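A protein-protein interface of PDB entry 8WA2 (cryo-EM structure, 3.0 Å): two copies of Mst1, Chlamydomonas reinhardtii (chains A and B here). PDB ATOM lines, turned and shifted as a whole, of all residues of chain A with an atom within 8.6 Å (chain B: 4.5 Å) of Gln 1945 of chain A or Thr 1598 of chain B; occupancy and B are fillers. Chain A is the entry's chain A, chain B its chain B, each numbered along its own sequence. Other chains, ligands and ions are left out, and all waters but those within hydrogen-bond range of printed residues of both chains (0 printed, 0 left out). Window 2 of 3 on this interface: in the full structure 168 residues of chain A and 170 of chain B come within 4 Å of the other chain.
O of Gln 1945 of chain A sits close to OD2 of Asp 1583 of chain B (3.5 Å). The guanidinium group of Arg 1622 of chain B sits at hydrogen-bond distance from the backbone carbonyl oxygen of Gln 1945 of chain A. O of Asn 1944 of chain A lies close to NH1 of Arg 1622 of chain B (3.4 Å). The side-chain hydroxyl (OG1) of Thr 1598 of chain B is in hydrogen-bond range of the side-chain amide oxygen (OE1) of Gln 1945 of chain A, 2.6 Å away. The side-chain amide oxygen (OD1) of Asn 1944 of chain A sits at hydrogen-bond distance from the backbone NH (N) of Asp 1583 of chain B (3.4 Å). The guanidinium group (NH1) of Arg 1622 of chain B sits close to the backbone carbonyl oxygen (O) of Asn 1946 of chain A (2.3 Å).
OE1 of Gln 1597 of chain B is in hydrogen-bond range of NZ of Lys 1658 of chain B. The backbone carbonyl oxygen of Gln 1597 of chain B is in hydrogen-bond range of the side-chain hydroxyl of Thr 1600 of chain B, 2.8 Å away. The side-chain amino group of Lys 1658 of chain B sits at hydrogen-bond distance from the backbone carbonyl oxygen of Thr 1598 of chain B (3.1 Å).
Among the printed residues, merely in contact across the chains: Asn 1946 of chain A with Asp 1583 of chain B (3.5 Å), Asn 1944 of chain A with Gln 1597 of chain B (3.6 Å) and Gln 1945 of chain A with Gln 1597 of chain B (3.9 Å).
Of the printed residues of chain B, Asn 1944 of chain A touches Asp 1583, Gln 1597 and Arg 1622. Gln 1945 of chain A touches just these residues of chain B: Asp 1583, Gln 1597, Thr 1598 and Arg 1622. Of the printed residues of chain B, Asn 1946 of chain A touches Asp 1583 (3.5 Å) and Arg 1622 (2.3 Å). Printed residues of chain A within 4 Å of Asp 1583 of chain B: Asn 1944, Gln 1945 and Asn 1946. Gln 1597 of chain B touches just these residues of chain A: Asn 1944 and Gln 1945. Of chain A, only Gln 1945 (2.6 Å) comes within 4 Å of Thr 1598 of chain B. No residue of chain A comes within 4 Å of Gly 1599 of chain B. Of the printed residues of chain A, Arg 1622 of chain B touches Asn 1944, Gln 1945 and Asn 1946. Lys 1658 of chain B touches none of the printed residues of chain A. The nearest printed residue of chain A that does not touch Asp 1583 of chain B is Gly 1947 of chain A (6.5 Å).
Along chain A the printed residues that touch a printed residue of chain B span positions 1944 to 1946. Among the printed residues, no Asp or Glu carboxylate lies within 4 Å of a Lys or Arg side-chain nitrogen of the other chain.
No position is printed for both chains. Of the 9 pairs that touch across the chains among the printed residues, none has its exchanged pair printed and touching as well.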
ATOM      1  N   GLY A1942     -12.296  -0.588  -7.224  1.00  0.00           N
ATOM      2  CA  GLY A1942     -12.200   0.659  -7.947  1.00  0.00           C
ATOM      3  C   GLY A1942     -11.817   0.527  -9.401  1.00  0.00           C
ATOM      4  O   GLY A1942     -11.657   1.550 -10.076  1.00  0.00           O
ATOM      5  N   VAL A1943     -11.664  -0.691  -9.906  1.00  0.00           N
ATOM      6  CA  VAL A1943     -11.274  -0.919 -11.291  1.00  0.00           C
ATOM      7  C   VAL A1943     -12.536  -1.133 -12.110  1.00  0.00           C
ATOM      8  O   VAL A1943     -13.259  -2.114 -11.908  1.00  0.00           O
ATOM      9  CB  VAL A1943     -10.330  -2.122 -11.412  1.00  0.00           C
ATOM     10  CG1 VAL A1943     -10.039  -2.421 -12.865  1.00  0.00           C
ATOM     11  CG2 VAL A1943      -9.047  -1.858 -10.657  1.00  0.00           C
ATOM     12  N   ASN A1944     -12.795  -0.223 -13.040  1.00  0.00           N
ATOM     13  CA  ASN A1944     -13.969  -0.320 -13.887  1.00  0.00           C
ATOM     14  C   ASN A1944     -13.656  -1.166 -15.113  1.00  0.00           C
ATOM     15  O   ASN A1944     -12.501  -1.460 -15.419  1.00  0.00           O
ATOM     16  CB  ASN A1944     -14.454   1.064 -14.298  1.00  0.00           C
ATOM     17  CG  ASN A1944     -15.919   1.081 -14.645  1.00  0.00           C
ATOM     18  OD1 ASN A1944     -16.610   0.074 -14.513  1.00  0.00           O
ATOM     19  ND2 ASN A1944     -16.408   2.232 -15.082  1.00  0.00           N
ATOM     20  N   GLN A1945     -14.714  -1.576 -15.805  1.00  0.00           N
ATOM     21  CA  GLN A1945     -14.669  -2.548 -16.892  1.00  0.00           C
ATOM     22  C   GLN A1945     -14.186  -3.913 -16.420  1.00  0.00           C
ATOM     23  O   GLN A1945     -13.835  -4.761 -17.248  1.00  0.00           O
ATOM     24  CB  GLN A1945     -13.806  -2.065 -18.069  1.00  0.00           C
ATOM     25  CG  GLN A1945     -14.219  -2.648 -19.410  1.00  0.00           C
ATOM     26  CD  GLN A1945     -13.095  -2.656 -20.414  1.00  0.00           C
ATOM     27  OE1 GLN A1945     -12.029  -2.094 -20.176  1.00  0.00           O
ATOM     28  NE2 GLN A1945     -13.330  -3.292 -21.553  1.00  0.00           N
ATOM     29  N   ASN A1946     -14.167  -4.147 -15.105  1.00  0.00           N
ATOM     30  CA  ASN A1946     -13.677  -5.392 -14.526  1.00  0.00           C
ATOM     31  C   ASN A1946     -12.266  -5.703 -15.007  1.00  0.00           C
ATOM     32  O   ASN A1946     -11.573  -4.825 -15.530  1.00  0.00           O
ATOM     33  CB  ASN A1946     -14.624  -6.549 -14.849  1.00  0.00           C
ATOM     34  CG  ASN A1946     -15.867  -6.537 -13.987  1.00  0.00           C
ATOM     35  OD1 ASN A1946     -16.134  -5.568 -13.280  1.00  0.00           O
ATOM     36  ND2 ASN A1946     -16.630  -7.621 -14.034  1.00  0.00           N
ATOM     37  N   GLY A1947     -11.819  -6.938 -14.819  1.00  0.00           N
ATOM     38  CA  GLY A1947     -10.477  -7.297 -15.236  1.00  0.00           C
ATOM     39  C   GLY A1947     -10.209  -8.760 -14.976  1.00  0.00           C
ATOM     40  O   GLY A1947     -11.056  -9.492 -14.453  1.00  0.00           O
ATOM     41  N   ASP A1948      -9.009  -9.177 -15.365  1.00  0.00           N
ATOM     42  CA  ASP A1948      -8.603 -10.559 -15.173  1.00  0.00           C
ATOM     43  C   ASP A1948      -8.525 -10.871 -13.682  1.00  0.00           C
ATOM     44  O   ASP A1948      -8.063 -10.035 -12.897  1.00  0.00           O
ATOM     45  CB  ASP A1948      -7.248 -10.816 -15.832  1.00  0.00           C
ATOM     46  CG  ASP A1948      -7.158 -10.239 -17.228  1.00  0.00           C
ATOM     47  OD1 ASP A1948      -7.955 -10.650 -18.097  1.00  0.00           O
ATOM     48  OD2 ASP A1948      -6.285  -9.380 -17.462  1.00  0.00           O
ATOM     49  N   ASP B1583     -19.504  -1.687 -14.841  1.00  0.00           N
ATOM     50  CA  ASP B1583     -19.870  -3.089 -14.986  1.00  0.00           C
ATOM     51  C   ASP B1583     -20.736  -3.560 -13.817  1.00  0.00           C
ATOM     52  O   ASP B1583     -21.030  -2.822 -12.874  1.00  0.00           O
ATOM     53  CB  ASP B1583     -18.630  -3.961 -15.143  1.00  0.00           C
ATOM     54  CG  ASP B1583     -18.369  -4.335 -16.588  1.00  0.00           C
ATOM     55  OD1 ASP B1583     -19.311  -4.817 -17.251  1.00  0.00           O
ATOM     56  OD2 ASP B1583     -17.240  -4.143 -17.070  1.00  0.00           O
ATOM     57  N   CYS B1596     -11.954   5.145 -15.725  1.00  0.00           N
ATOM     58  CA  CYS B1596     -12.713   5.221 -16.962  1.00  0.00           C
ATOM     59  C   CYS B1596     -12.491   3.961 -17.788  1.00  0.00           C
ATOM     60  O   CYS B1596     -11.369   3.461 -17.894  1.00  0.00           O
ATOM     61  CB  CYS B1596     -12.307   6.453 -17.767  1.00  0.00           C
ATOM     62  SG  CYS B1596     -12.898   8.014 -17.093  1.00  0.00           S
ATOM     63  N   GLN B1597     -13.570   3.453 -18.376  1.00  0.00           N
ATOM     64  CA  GLN B1597     -13.485   2.252 -19.188  1.00  0.00           C
ATOM     65  C   GLN B1597     -12.589   2.486 -20.402  1.00  0.00           C
ATOM     66  O   GLN B1597     -12.231   3.614 -20.741  1.00  0.00           O
ATOM     67  CB  GLN B1597     -14.874   1.826 -19.653  1.00  0.00           C
ATOM     68  CG  GLN B1597     -15.781   1.341 -18.553  1.00  0.00           C
ATOM     69  CD  GLN B1597     -16.828   0.387 -19.067  1.00  0.00           C
ATOM     70  OE1 GLN B1597     -16.876   0.087 -20.258  1.00  0.00           O
ATOM     71  NE2 GLN B1597     -17.678  -0.095 -18.172  1.00  0.00           N
ATOM     72  N   THR B1598     -12.231   1.392 -21.067  1.00  0.00           N
ATOM     73  CA  THR B1598     -11.508   1.502 -22.324  1.00  0.00           C
ATOM     74  C   THR B1598     -12.425   2.093 -23.384  1.00  0.00           C
ATOM     75  O   THR B1598     -13.599   1.730 -23.484  1.00  0.00           O
ATOM     76  CB  THR B1598     -10.996   0.140 -22.778  1.00  0.00           C
ATOM     77  OG1 THR B1598     -11.992  -0.854 -22.515  1.00  0.00           O
ATOM     78  CG2 THR B1598      -9.726  -0.221 -22.034  1.00  0.00           C
ATOM     79  N   GLY B1599     -11.884   3.011 -24.178  1.00  0.00           N
ATOM     80  CA  GLY B1599     -12.682   3.779 -25.102  1.00  0.00           C
ATOM     81  C   GLY B1599     -13.201   5.087 -24.550  1.00  0.00           C
ATOM     82  O   GLY B1599     -13.772   5.878 -25.310  1.00  0.00           O
ATOM     83  N   THR B1600     -13.025   5.340 -23.255  1.00  0.00           N
ATOM     84  CA  THR B1600     -13.417   6.594 -22.636  1.00  0.00           C
ATOM     85  C   THR B1600     -12.237   7.152 -21.854  1.00  0.00           C
ATOM     86  O   THR B1600     -11.333   6.419 -21.448  1.00  0.00           O
ATOM     87  CB  THR B1600     -14.622   6.426 -21.704  1.00  0.00           C
ATOM     88  OG1 THR B1600     -14.371   5.354 -20.788  1.00  0.00           O
ATOM     89  CG2 THR B1600     -15.870   6.109 -22.504  1.00  0.00           C
ATOM     90  N   ALA B1619      -8.671   4.870 -26.714  1.00  0.00           N
ATOM     91  CA  ALA B1619      -8.234   4.676 -25.335  1.00  0.00           C
ATOM     92  C   ALA B1619      -8.051   3.179 -25.123  1.00  0.00           C
ATOM     93  O   ALA B1619      -9.028   2.449 -24.930  1.00  0.00           O
ATOM     94  CB  ALA B1619      -9.241   5.260 -24.353  1.00  0.00           C
ATOM     95  N   SER B1620      -6.802   2.723 -25.154  1.00  0.00           N
ATOM     96  CA  SER B1620      -6.509   1.302 -25.047  1.00  0.00           C
ATOM     97  C   SER B1620      -6.324   0.833 -23.613  1.00  0.00           C
ATOM     98  O   SER B1620      -6.442  -0.370 -23.350  1.00  0.00           O
ATOM     99  CB  SER B1620      -5.253   0.962 -25.854  1.00  0.00           C
ATOM    100  OG  SER B1620      -4.280   1.982 -25.723  1.00  0.00           O
ATOM    101  N   LYS B1621      -6.034   1.737 -22.687  1.00  0.00           N
ATOM    102  CA  LYS B1621      -5.835   1.386 -21.294  1.00  0.00           C
ATOM    103  C   LYS B1621      -7.016   1.867 -20.461  1.00  0.00           C
ATOM    104  O   LYS B1621      -8.011   2.379 -20.982  1.00  0.00           O
ATOM    105  CB  LYS B1621      -4.514   1.962 -20.785  1.00  0.00           C
ATOM    106  CG  LYS B1621      -3.320   1.646 -21.660  1.00  0.00           C
ATOM    107  CD  LYS B1621      -2.689   0.332 -21.250  1.00  0.00           C
ATOM    108  CE  LYS B1621      -1.381   0.095 -21.977  1.00  0.00           C
ATOM    109  NZ  LYS B1621      -1.427   0.515 -23.403  1.00  0.00           N
ATOM    110  N   ARG B1622      -6.906   1.709 -19.149  1.00  0.00           N
ATOM    111  CA  ARG B1622      -7.980   2.012 -18.219  1.00  0.00           C
ATOM    112  C   ARG B1622      -7.627   3.250 -17.410  1.00  0.00           C
ATOM    113  O   ARG B1622      -6.478   3.422 -16.992  1.00  0.00           O
ATOM    114  CB  ARG B1622      -8.229   0.827 -17.288  1.00  0.00           C
ATOM    115  CG  ARG B1622      -9.576   0.166 -17.466  1.00  0.00           C
ATOM    116  CD  ARG B1622      -9.665  -1.085 -16.618  1.00  0.00           C
ATOM    117  NE  ARG B1622      -8.916  -2.193 -17.198  1.00  0.00           N
ATOM    118  CZ  ARG B1622      -9.438  -3.373 -17.500  1.00  0.00           C
ATOM    119  NH1 ARG B1622     -10.716  -3.638 -17.286  1.00  0.00           N
ATOM    120  NH2 ARG B1622      -8.659  -4.310 -18.029  1.00  0.00           N
ATOM    121  N   LYS B1658     -19.177   4.700 -25.661  1.00  0.00           N
ATOM    122  CA  LYS B1658     -17.724   4.771 -25.684  1.00  0.00           C
ATOM    123  C   LYS B1658     -17.191   4.785 -27.114  1.00  0.00           C
ATOM    124  O   LYS B1658     -17.886   4.450 -28.077  1.00  0.00           O
ATOM    125  CB  LYS B1658     -17.121   3.597 -24.915  1.00  0.00           C
ATOM    126  CG  LYS B1658     -17.427   2.241 -25.515  1.00  0.00           C
ATOM    127  CD  LYS B1658     -17.399   1.153 -24.458  1.00  0.00           C
ATOM    128  CE  LYS B1658     -16.258   0.183 -24.706  1.00  0.00           C
ATOM    129  NZ  LYS B1658     -15.819  -0.487 -23.453  1.00  0.00           N
ATOM    130  N   GLN B1661     -11.260   1.169 -28.721  1.00  0.00           N
ATOM    131  CA  GLN B1661     -10.163   0.700 -27.885  1.00  0.00           C
ATOM    132  C   GLN B1661      -8.860   0.567 -28.660  1.00  0.00           C
ATOM    133  O   GLN B1661      -7.786   0.849 -28.118  1.00  0.00           O
ATOM    134  CB  GLN B1661     -10.518  -0.645 -27.252  1.00  0.00           C
ATOM    135  CG  GLN B1661     -11.959  -0.765 -26.821  1.00  0.00           C
ATOM    136  CD  GLN B1661     -12.260  -2.117 -26.214  1.00  0.00           C
ATOM    137  OE1 GLN B1661     -11.407  -3.004 -26.196  1.00  0.00           O
ATOM    138  NE2 GLN B1661     -13.478  -2.283 -25.712  1.00  0.00           N
